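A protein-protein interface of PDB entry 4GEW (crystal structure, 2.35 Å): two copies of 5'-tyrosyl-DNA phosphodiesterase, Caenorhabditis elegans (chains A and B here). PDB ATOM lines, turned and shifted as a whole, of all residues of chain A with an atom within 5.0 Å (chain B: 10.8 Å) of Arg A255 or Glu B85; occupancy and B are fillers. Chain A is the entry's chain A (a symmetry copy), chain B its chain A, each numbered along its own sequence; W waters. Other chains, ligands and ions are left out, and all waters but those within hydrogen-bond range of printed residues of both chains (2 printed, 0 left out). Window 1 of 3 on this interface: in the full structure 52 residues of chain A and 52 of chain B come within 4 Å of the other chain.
NE of Arg A255 is in salt-bridge range of OE2 of Glu B85 (3.7 Å).
OD1 of Asp A252 is in salt-bridge range of NH2 of Arg B91 (2.7 Å).
The backbone carbonyl oxygen (O) of Ala A259 lies close to the backbone carbonyl oxygen (O) of Ala B259, 3.5 Å away.
O of Phe B81 sits at hydrogen-bond distance from NH1 of Arg B91, at 2.7 Å.
The backbone carbonyl oxygen (O) of Tyr B82 lies close to the guanidinium group (NH1) of Arg B91 (3.5 Å).
The backbone carbonyl oxygen (O) of Ser B84 sits at hydrogen-bond distance from the guanidinium group (NH1) of Arg B91, 2.8 Å away.
The guanidinium group of Arg B91 is in hydrogen-bond range of the backbone carbonyl oxygen of Phe B87, 3.4 Å away.
The side-chain carboxylate of Asp A252 is in salt-bridge range of the guanidinium group of Arg A255.
Among the printed residues, merely in contact across the chains: Asp A252 with Ala B88 (3.7 Å), Arg A255 with Ala B88 (3.9 Å) and Ala A259 with Gln B260 (3.6 Å).
Arg A255 touches just these residues of chain B: Glu B85 (3.4 Å) and Ala B88 (3.9 Å).
Glu B85 touches just one residue of chain A: Arg A255 (3.4 Å).
Of chain B, only Ala B88 and Arg B91 come within 4 Å of Asp A252.
No residue of chain B comes within 4 Å of Val A254.
No residue of chain B comes within 4 Å of Glu A256.
No residue of chain B comes within 4 Å of Ile A257.
No residue of chain B comes within 4 Å of Ile A258.
Of the printed residues of chain B, Ala A259 touches Ala B259 (3.5 Å) and Gln B260 (3.6 Å).
Of the printed residues of chain A, Ala B88 touches Asp A252 (3.7 Å) and Arg A255 (3.9 Å).
Of the printed residues of chain A, Ala B259 touches Ala A259.
Printed residues of chain A within 4 Å of Arg B91: Asp A252 (2.7 Å).
Printed residues of chain A within 4 Å of Gln B260: Ala A259 (3.6 Å).
Lys A253 touches none of the printed residues of chain B.
Ala B77 touches none of the printed residues of chain A.
The nearest printed residue of chain A that does not touch Glu B85 is Asp A252 (5.5 Å).
Of the 10 printed residues of chain A, 3 touch a printed residue of chain B.
Printed residues of chain B that touch a printed residue of chain A: Glu B85, Ala B88, Arg B91, Ala B259 and Gln B260.
Hydrophobic or aromatic side chains of chain B within 4 Å of the printed part of chain A: Ala B88.
Among the printed residues, 6 pairs touch across the chains.
Among the printed residues, Asp or Glu carboxylates within 4 Å of a Lys or Arg side-chain nitrogen of the other chain: Asp A252 with Arg B91 (2.7 Å) and Arg A255 with Glu B85 (3.7 Å).
Ala B259 touches its own counterpart, Ala A259.
Positions printed for both chains: 258 and 259.
Of the 6 pairs that touch across the chains among the printed residues, 1 has its exchanged pair printed and touching as well.
Water W2 lies within hydrogen-bond range of OD2 of Asp A252 (2.5 Å), O of Ala B88 (2.7 Å) and N of Ser B92 (3.5 Å).
Water W1 bridges O of Tyr B82 (2.8 Å) and OD1 of Asp A252 (3.4 Å).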
ATOM      1  N   MET A 251       6.606 -13.452   6.096  1.00  0.00           N
ATOM      2  CA  MET A 251       7.544 -14.310   6.813  1.00  0.00           C
ATOM      3  C   MET A 251       8.845 -13.577   7.117  1.00  0.00           C
ATOM      4  O   MET A 251       9.512 -13.885   8.099  1.00  0.00           O
ATOM      5  CB  MET A 251       7.802 -15.619   6.061  1.00  0.00           C
ATOM      6  CG  MET A 251       6.667 -16.633   6.201  1.00  0.00           C
ATOM      7  SD  MET A 251       6.291 -17.029   7.930  1.00  0.00           S
ATOM      8  CE  MET A 251       4.931 -18.175   7.736  1.00  0.00           C
ATOM      9  N   ASP A 252       9.202 -12.603   6.285  1.00  0.00           N
ATOM     10  CA  ASP A 252      10.351 -11.753   6.586  1.00  0.00           C
ATOM     11  C   ASP A 252      10.086 -10.956   7.857  1.00  0.00           C
ATOM     12  O   ASP A 252      10.961 -10.826   8.709  1.00  0.00           O
ATOM     13  CB  ASP A 252      10.657 -10.797   5.424  1.00  0.00           C
ATOM     14  CG  ASP A 252      11.180 -11.514   4.186  1.00  0.00           C
ATOM     15  OD1 ASP A 252      11.759 -12.609   4.331  1.00  0.00           O
ATOM     16  OD2 ASP A 252      11.019 -10.968   3.068  1.00  0.00           O
ATOM     17  N   LYS A 253       8.872 -10.427   7.983  1.00  0.00           N
ATOM     18  CA  LYS A 253       8.491  -9.638   9.153  1.00  0.00           C
ATOM     19  C   LYS A 253       8.485 -10.491  10.416  1.00  0.00           C
ATOM     20  O   LYS A 253       8.976 -10.064  11.462  1.00  0.00           O
ATOM     21  CB  LYS A 253       7.127  -8.979   8.929  1.00  0.00           C
ATOM     22  CG  LYS A 253       7.199  -7.542   8.399  1.00  0.00           C
ATOM     23  CD  LYS A 253       8.248  -7.380   7.299  1.00  0.00           C
ATOM     24  CE  LYS A 253       8.830  -5.968   7.269  1.00  0.00           C
ATOM     25  NZ  LYS A 253      10.002  -5.875   6.338  1.00  0.00           N
ATOM     26  N   VAL A 254       7.950 -11.705  10.304  1.00  0.00           N
ATOM     27  CA  VAL A 254       7.963 -12.646  11.418  1.00  0.00           C
ATOM     28  C   VAL A 254       9.398 -12.926  11.849  1.00  0.00           C
ATOM     29  O   VAL A 254       9.717 -12.910  13.039  1.00  0.00           O
ATOM     30  CB  VAL A 254       7.262 -13.961  11.039  1.00  0.00           C
ATOM     31  CG1 VAL A 254       7.527 -15.038  12.076  1.00  0.00           C
ATOM     32  CG2 VAL A 254       5.756 -13.721  10.867  1.00  0.00           C
ATOM     33  N   ARG A 255      10.265 -13.155  10.869  1.00  0.00           N
ATOM     34  CA  ARG A 255      11.672 -13.428  11.128  1.00  0.00           C
ATOM     35  C   ARG A 255      12.358 -12.260  11.847  1.00  0.00           C
ATOM     36  O   ARG A 255      13.218 -12.476  12.696  1.00  0.00           O
ATOM     37  CB  ARG A 255      12.391 -13.756   9.817  1.00  0.00           C
ATOM     38  CG  ARG A 255      13.643 -14.589   9.992  1.00  0.00           C
ATOM     39  CD  ARG A 255      14.350 -14.836   8.668  1.00  0.00           C
ATOM     40  NE  ARG A 255      14.743 -13.587   8.023  1.00  0.00           N
ATOM     41  CZ  ARG A 255      14.228 -13.145   6.881  1.00  0.00           C
ATOM     42  NH1 ARG A 255      13.310 -13.862   6.250  1.00  0.00           N
ATOM     43  NH2 ARG A 255      14.640 -11.994   6.365  1.00  0.00           N
ATOM     44  N   GLU A 256      11.973 -11.028  11.511  1.00  0.00           N
ATOM     45  CA  GLU A 256      12.549  -9.844  12.154  1.00  0.00           C
ATOM     46  C   GLU A 256      12.099  -9.726  13.606  1.00  0.00           C
ATOM     47  O   GLU A 256      12.902  -9.450  14.498  1.00  0.00           O
ATOM     48  CB  GLU A 256      12.159  -8.568  11.411  1.00  0.00           C
ATOM     49  CG  GLU A 256      12.777  -8.419  10.035  1.00  0.00           C
ATOM     50  CD  GLU A 256      12.420  -7.093   9.387  1.00  0.00           C
ATOM     51  OE1 GLU A 256      11.606  -6.346   9.974  1.00  0.00           O
ATOM     52  OE2 GLU A 256      12.956  -6.799   8.295  1.00  0.00           O
ATOM     53  N   ILE A 257      10.803  -9.916  13.826  1.00  0.00           N
ATOM     54  CA  ILE A 257      10.232  -9.870  15.164  1.00  0.00           C
ATOM     55  C   ILE A 257      10.878 -10.912  16.079  1.00  0.00           C
ATOM     56  O   ILE A 257      11.236 -10.611  17.220  1.00  0.00           O
ATOM     57  CB  ILE A 257       8.703 -10.063  15.106  1.00  0.00           C
ATOM     58  CG1 ILE A 257       8.055  -8.846  14.429  1.00  0.00           C
ATOM     59  CG2 ILE A 257       8.131 -10.313  16.502  1.00  0.00           C
ATOM     60  CD1 ILE A 257       6.570  -8.992  14.157  1.00  0.00           C
ATOM     61  N   ILE A 258      11.052 -12.128  15.570  1.00  0.00           N
ATOM     62  CA  ILE A 258      11.667 -13.197  16.355  1.00  0.00           C
ATOM     63  C   ILE A 258      13.109 -12.861  16.727  1.00  0.00           C
ATOM     64  O   ILE A 258      13.530 -13.075  17.860  1.00  0.00           O
ATOM     65  CB  ILE A 258      11.624 -14.547  15.610  1.00  0.00           C
ATOM     66  CG1 ILE A 258      10.176 -15.015  15.448  1.00  0.00           C
ATOM     67  CG2 ILE A 258      12.455 -15.604  16.349  1.00  0.00           C
ATOM     68  CD1 ILE A 258      10.029 -16.191  14.520  1.00  0.00           C
ATOM     69  N   ALA A 259      13.858 -12.320  15.771  1.00  0.00           N
ATOM     70  CA  ALA A 259      15.260 -11.980  16.003  1.00  0.00           C
ATOM     71  C   ALA A 259      15.407 -10.879  17.044  1.00  0.00           C
ATOM     72  O   ALA A 259      16.351 -10.879  17.832  1.00  0.00           O
ATOM     73  CB  ALA A 259      15.932 -11.566  14.702  1.00  0.00           C
ATOM     74  N   PRO A 283      10.514 -19.551   8.343  1.00  0.00           N
ATOM     75  CA  PRO A 283      11.725 -19.338   9.149  1.00  0.00           C
ATOM     76  C   PRO A 283      11.892 -20.352  10.290  1.00  0.00           C
ATOM     77  O   PRO A 283      10.928 -21.002  10.689  1.00  0.00           O
ATOM     78  CB  PRO A 283      11.544 -17.915   9.698  1.00  0.00           C
ATOM     79  CG  PRO A 283      10.093 -17.596   9.524  1.00  0.00           C
ATOM     80  CD  PRO A 283       9.639 -18.367   8.325  1.00  0.00           C
ATOM     81  N   LYS B  76      14.515 -24.204  -7.830  1.00  0.00           N
ATOM     82  CA  LYS B  76      15.157 -23.668  -6.636  1.00  0.00           C
ATOM     83  C   LYS B  76      15.423 -22.167  -6.757  1.00  0.00           C
ATOM     84  O   LYS B  76      15.693 -21.495  -5.763  1.00  0.00           O
ATOM     85  CB  LYS B  76      16.427 -24.452  -6.275  1.00  0.00           C
ATOM     86  CG  LYS B  76      17.576 -24.315  -7.245  1.00  0.00           C
ATOM     87  CD  LYS B  76      18.772 -25.147  -6.790  1.00  0.00           C
ATOM     88  CE  LYS B  76      18.570 -26.631  -7.054  1.00  0.00           C
ATOM     89  NZ  LYS B  76      19.857 -27.302  -7.397  1.00  0.00           N
ATOM     90  N   ALA B  77      15.328 -21.641  -7.974  1.00  0.00           N
ATOM     91  CA  ALA B  77      15.386 -20.198  -8.177  1.00  0.00           C
ATOM     92  C   ALA B  77      14.136 -19.553  -7.579  1.00  0.00           C
ATOM     93  O   ALA B  77      14.209 -18.486  -6.967  1.00  0.00           O
ATOM     94  CB  ALA B  77      15.508 -19.868  -9.656  1.00  0.00           C
ATOM     95  N   LEU B  78      12.994 -20.214  -7.760  1.00  0.00           N
ATOM     96  CA  LEU B  78      11.740 -19.771  -7.154  1.00  0.00           C
ATOM     97  C   LEU B  78      11.806 -19.831  -5.634  1.00  0.00           C
ATOM     98  O   LEU B  78      11.443 -18.871  -4.951  1.00  0.00           O
ATOM     99  CB  LEU B  78      10.560 -20.619  -7.645  1.00  0.00           C
ATOM    100  CG  LEU B  78       9.811 -20.211  -8.920  1.00  0.00           C
ATOM    101  CD1 LEU B  78      10.179 -18.810  -9.362  1.00  0.00           C
ATOM    102  CD2 LEU B  78      10.055 -21.205 -10.042  1.00  0.00           C
ATOM    103  N   ASP B  79      12.264 -20.967  -5.111  1.00  0.00           N
ATOM    104  CA  ASP B  79      12.369 -21.167  -3.667  1.00  0.00           C
ATOM    105  C   ASP B  79      13.272 -20.113  -3.040  1.00  0.00           C
ATOM    106  O   ASP B  79      13.008 -19.626  -1.941  1.00  0.00           O
ATOM    107  CB  ASP B  79      12.904 -22.565  -3.348  1.00  0.00           C
ATOM    108  CG  ASP B  79      12.028 -23.671  -3.911  1.00  0.00           C
ATOM    109  OD1 ASP B  79      12.516 -24.817  -4.029  1.00  0.00           O
ATOM    110  OD2 ASP B  79      10.855 -23.393  -4.239  1.00  0.00           O
ATOM    111  N   VAL B  80      14.339 -19.767  -3.753  1.00  0.00           N
ATOM    112  CA  VAL B  80      15.266 -18.736  -3.307  1.00  0.00           C
ATOM    113  C   VAL B  80      14.604 -17.358  -3.288  1.00  0.00           C
ATOM    114  O   VAL B  80      14.727 -16.617  -2.315  1.00  0.00           O
ATOM    115  CB  VAL B  80      16.539 -18.709  -4.188  1.00  0.00           C
ATOM    116  CG1 VAL B  80      17.210 -17.348  -4.139  1.00  0.00           C
ATOM    117  CG2 VAL B  80      17.506 -19.802  -3.754  1.00  0.00           C
ATOM    118  N   PHE B  81      13.896 -17.014  -4.355  1.00  0.00           N
ATOM    119  CA  PHE B  81      13.245 -15.711  -4.410  1.00  0.00           C
ATOM    120  C   PHE B  81      12.243 -15.525  -3.268  1.00  0.00           C
ATOM    121  O   PHE B  81      12.217 -14.478  -2.624  1.00  0.00           O
ATOM    122  CB  PHE B  81      12.562 -15.479  -5.758  1.00  0.00           C
ATOM    123  CG  PHE B  81      11.785 -14.199  -5.815  1.00  0.00           C
ATOM    124  CD1 PHE B  81      12.436 -12.978  -5.782  1.00  0.00           C
ATOM    125  CD2 PHE B  81      10.401 -14.214  -5.888  1.00  0.00           C
ATOM    126  CE1 PHE B  81      11.727 -11.796  -5.825  1.00  0.00           C
ATOM    127  CE2 PHE B  81       9.686 -13.033  -5.933  1.00  0.00           C
ATOM    128  CZ  PHE B  81      10.350 -11.822  -5.901  1.00  0.00           C
ATOM    129  N   TYR B  82      11.438 -16.549  -3.008  1.00  0.00           N
ATOM    130  CA  TYR B  82      10.391 -16.444  -1.995  1.00  0.00           C
ATOM    131  C   TYR B  82      10.861 -16.778  -0.585  1.00  0.00           C
ATOM    132  O   TYR B  82      10.393 -16.178   0.378  1.00  0.00           O
ATOM    133  CB  TYR B  82       9.185 -17.314  -2.364  1.00  0.00           C
ATOM    134  CG  TYR B  82       8.461 -16.832  -3.595  1.00  0.00           C
ATOM    135  CD1 TYR B  82       7.893 -15.569  -3.633  1.00  0.00           C
ATOM    136  CD2 TYR B  82       8.343 -17.637  -4.717  1.00  0.00           C
ATOM    137  CE1 TYR B  82       7.231 -15.113  -4.758  1.00  0.00           C
ATOM    138  CE2 TYR B  82       7.680 -17.189  -5.851  1.00  0.00           C
ATOM    139  CZ  TYR B  82       7.124 -15.924  -5.863  1.00  0.00           C
ATOM    140  OH  TYR B  82       6.462 -15.461  -6.984  1.00  0.00           O
ATOM    141  N   GLY B  83      11.784 -17.728  -0.464  1.00  0.00           N
ATOM    142  CA  GLY B  83      12.151 -18.251   0.840  1.00  0.00           C
ATOM    143  C   GLY B  83      13.501 -17.835   1.395  1.00  0.00           C
ATOM    144  O   GLY B  83      13.669 -17.753   2.615  1.00  0.00           O
ATOM    145  N   SER B  84      14.469 -17.588   0.518  1.00  0.00           N
ATOM    146  CA  SER B  84      15.823 -17.271   0.968  1.00  0.00           C
ATOM    147  C   SER B  84      15.908 -15.915   1.660  1.00  0.00           C
ATOM    148  O   SER B  84      15.287 -14.940   1.238  1.00  0.00           O
ATOM    149  CB  SER B  84      16.825 -17.334  -0.188  1.00  0.00           C
ATOM    150  OG  SER B  84      18.106 -16.905   0.239  1.00  0.00           O
ATOM    151  N   GLU B  85      16.703 -15.863   2.722  1.00  0.00           N
ATOM    152  CA  GLU B  85      16.830 -14.665   3.539  1.00  0.00           C
ATOM    153  C   GLU B  85      17.622 -13.577   2.823  1.00  0.00           C
ATOM    154  O   GLU B  85      17.489 -12.399   3.138  1.00  0.00           O
ATOM    155  CB  GLU B  85      17.491 -15.028   4.865  1.00  0.00           C
ATOM    156  CG  GLU B  85      17.431 -13.938   5.919  1.00  0.00           C
ATOM    157  CD  GLU B  85      18.164 -14.327   7.185  1.00  0.00           C
ATOM    158  OE1 GLU B  85      18.465 -15.530   7.352  1.00  0.00           O
ATOM    159  OE2 GLU B  85      18.448 -13.432   8.009  1.00  0.00           O
ATOM    160  N   ALA B  86      18.436 -13.977   1.854  1.00  0.00           N
ATOM    161  CA  ALA B  86      19.233 -13.028   1.087  1.00  0.00           C
ATOM    162  C   ALA B  86      18.363 -12.084   0.255  1.00  0.00           C
ATOM    163  O   ALA B  86      18.767 -10.962  -0.051  1.00  0.00           O
ATOM    164  CB  ALA B  86      20.214 -13.771   0.189  1.00  0.00           C
ATOM    165  N   PHE B  87      17.169 -12.538  -0.107  1.00  0.00           N
ATOM    166  CA  PHE B  87      16.321 -11.779  -1.020  1.00  0.00           C
ATOM    167  C   PHE B  87      15.148 -11.080  -0.346  1.00  0.00           C
ATOM    168  O   PHE B  87      14.107 -10.871  -0.968  1.00  0.00           O
ATOM    169  CB  PHE B  87      15.829 -12.678  -2.152  1.00  0.00           C
ATOM    170  CG  PHE B  87      16.885 -12.987  -3.165  1.00  0.00           C
ATOM    171  CD1 PHE B  87      16.980 -12.244  -4.328  1.00  0.00           C
ATOM    172  CD2 PHE B  87      17.798 -14.005  -2.946  1.00  0.00           C
ATOM    173  CE1 PHE B  87      17.959 -12.518  -5.260  1.00  0.00           C
ATOM    174  CE2 PHE B  87      18.780 -14.283  -3.877  1.00  0.00           C
ATOM    175  CZ  PHE B  87      18.859 -13.540  -5.034  1.00  0.00           C
ATOM    176  N   ALA B  88      15.329 -10.703   0.915  1.00  0.00           N
ATOM    177  CA  ALA B  88      14.299  -9.982   1.650  1.00  0.00           C
ATOM    178  C   ALA B  88      14.074  -8.594   1.053  1.00  0.00           C
ATOM    179  O   ALA B  88      12.940  -8.118   0.975  1.00  0.00           O
ATOM    180  CB  ALA B  88      14.665  -9.885   3.127  1.00  0.00           C
ATOM    181  N   GLU B  89      15.157  -7.950   0.628  1.00  0.00           N
ATOM    182  CA  GLU B  89      15.053  -6.640  -0.002  1.00  0.00           C
ATOM    183  C   GLU B  89      14.254  -6.727  -1.298  1.00  0.00           C
ATOM    184  O   GLU B  89      13.433  -5.857  -1.591  1.00  0.00           O
ATOM    185  CB  GLU B  89      16.440  -6.058  -0.276  1.00  0.00           C
ATOM    186  CG  GLU B  89      17.236  -5.729   0.979  1.00  0.00           C
ATOM    187  CD  GLU B  89      16.651  -4.564   1.763  1.00  0.00           C
ATOM    188  OE1 GLU B  89      17.094  -3.416   1.536  1.00  0.00           O
ATOM    189  OE2 GLU B  89      15.757  -4.797   2.609  1.00  0.00           O
ATOM    190  N   ALA B  90      14.497  -7.786  -2.065  1.00  0.00           N
ATOM    191  CA  ALA B  90      13.806  -7.990  -3.331  1.00  0.00           C
ATOM    192  C   ALA B  90      12.317  -8.215  -3.106  1.00  0.00           C
ATOM    193  O   ALA B  90      11.484  -7.713  -3.857  1.00  0.00           O
ATOM    194  CB  ALA B  90      14.416  -9.163  -4.089  1.00  0.00           C
ATOM    195  N   ARG B  91      11.985  -8.967  -2.065  1.00  0.00           N
ATOM    196  CA  ARG B  91      10.588  -9.214  -1.736  1.00  0.00           C
ATOM    197  C   ARG B  91       9.908  -7.941  -1.234  1.00  0.00           C
ATOM    198  O   ARG B  91       8.736  -7.698  -1.514  1.00  0.00           O
ATOM    199  CB  ARG B  91      10.464 -10.343  -0.711  1.00  0.00           C
ATOM    200  CG  ARG B  91      10.787 -11.720  -1.273  1.00  0.00           C
ATOM    201  CD  ARG B  91      10.453 -12.829  -0.283  1.00  0.00           C
ATOM    202  NE  ARG B  91      11.302 -12.775   0.903  1.00  0.00           N
ATOM    203  CZ  ARG B  91      12.511 -13.321   0.981  1.00  0.00           C
ATOM    204  NH1 ARG B  91      13.020 -13.965  -0.061  1.00  0.00           N
ATOM    205  NH2 ARG B  91      13.215 -13.220   2.100  1.00  0.00           N
ATOM    206  N   SER B  92      10.654  -7.128  -0.495  1.00  0.00           N
ATOM    207  CA  SER B  92      10.126  -5.871   0.013  1.00  0.00           C
ATOM    208  C   SER B  92       9.845  -4.915  -1.139  1.00  0.00           C
ATOM    209  O   SER B  92       8.846  -4.198  -1.131  1.00  0.00           O
ATOM    210  CB  SER B  92      11.102  -5.242   1.011  1.00  0.00           C
ATOM    211  OG  SER B  92      10.613  -3.995   1.471  1.00  0.00           O
ATOM    212  N   ILE B 258      23.497  -7.185  18.420  1.00  0.00           N
ATOM    213  CA  ILE B 258      23.243  -6.697  17.066  1.00  0.00           C
ATOM    214  C   ILE B 258      21.905  -7.200  16.531  1.00  0.00           C
ATOM    215  O   ILE B 258      21.147  -6.445  15.928  1.00  0.00           O
ATOM    216  CB  ILE B 258      24.373  -7.097  16.096  1.00  0.00           C
ATOM    217  CG1 ILE B 258      25.677  -6.396  16.487  1.00  0.00           C
ATOM    218  CG2 ILE B 258      23.993  -6.764  14.648  1.00  0.00           C
ATOM    219  CD1 ILE B 258      26.881  -6.919  15.749  1.00  0.00           C
ATOM    220  N   ALA B 259      21.612  -8.475  16.767  1.00  0.00           N
ATOM    221  CA  ALA B 259      20.371  -9.075  16.280  1.00  0.00           C
ATOM    222  C   ALA B 259      19.149  -8.445  16.935  1.00  0.00           C
ATOM    223  O   ALA B 259      18.106  -8.288  16.302  1.00  0.00           O
ATOM    224  CB  ALA B 259      20.377 -10.578  16.514  1.00  0.00           C
ATOM    225  N   GLN B 260      19.286  -8.077  18.202  1.00  0.00           N
ATOM    226  CA  GLN B 260      18.164  -7.527  18.954  1.00  0.00           C
ATOM    227  C   GLN B 260      18.047  -6.009  18.852  1.00  0.00           C
ATOM    228  O   GLN B 260      17.022  -5.436  19.219  1.00  0.00           O
ATOM    229  CB  GLN B 260      18.254  -7.955  20.419  1.00  0.00           C
ATOM    230  CG  GLN B 260      18.175  -9.456  20.600  1.00  0.00           C
ATOM    231  CD  GLN B 260      18.480  -9.892  22.016  1.00  0.00           C
ATOM    232  OE1 GLN B 260      18.099  -9.229  22.982  1.00  0.00           O
ATOM    233  NE2 GLN B 260      19.174 -11.012  22.146  1.00  0.00           N
ATOM    234  N   PRO B 262      18.790  -3.571  15.859  1.00  0.00           N
ATOM    235  CA  PRO B 262      19.163  -3.009  14.555  1.00  0.00           C
ATOM    236  C   PRO B 262      19.338  -1.499  14.655  1.00  0.00           C
ATOM    237  O   PRO B 262      18.525  -0.828  15.295  1.00  0.00           O
ATOM    238  CB  PRO B 262      17.953  -3.336  13.667  1.00  0.00           C
ATOM    239  CG  PRO B 262      16.822  -3.546  14.618  1.00  0.00           C
ATOM    240  CD  PRO B 262      17.446  -4.173  15.838  1.00  0.00           C
ATOM    241  N   ASP B 284      29.023 -11.033  11.235  1.00  0.00           N
ATOM    242  CA  ASP B 284      28.756 -10.146  10.101  1.00  0.00           C
ATOM    243  C   ASP B 284      28.515  -8.701  10.534  1.00  0.00           C
ATOM    244  O   ASP B 284      27.797  -8.445  11.501  1.00  0.00           O
ATOM    245  CB  ASP B 284      27.548 -10.650   9.313  1.00  0.00           C
ATOM    246  CG  ASP B 284      27.708 -12.084   8.854  1.00  0.00           C
ATOM    247  OD1 ASP B 284      28.863 -12.552   8.772  1.00  0.00           O
ATOM    248  OD2 ASP B 284      26.684 -12.743   8.569  1.00  0.00           O
HETATM  249  O   HOH W   1      10.206 -15.358   3.084  1.00  0.00           O
HETATM  250  O   HOH W   2      10.891  -8.514   2.698  1.00  0.00           O
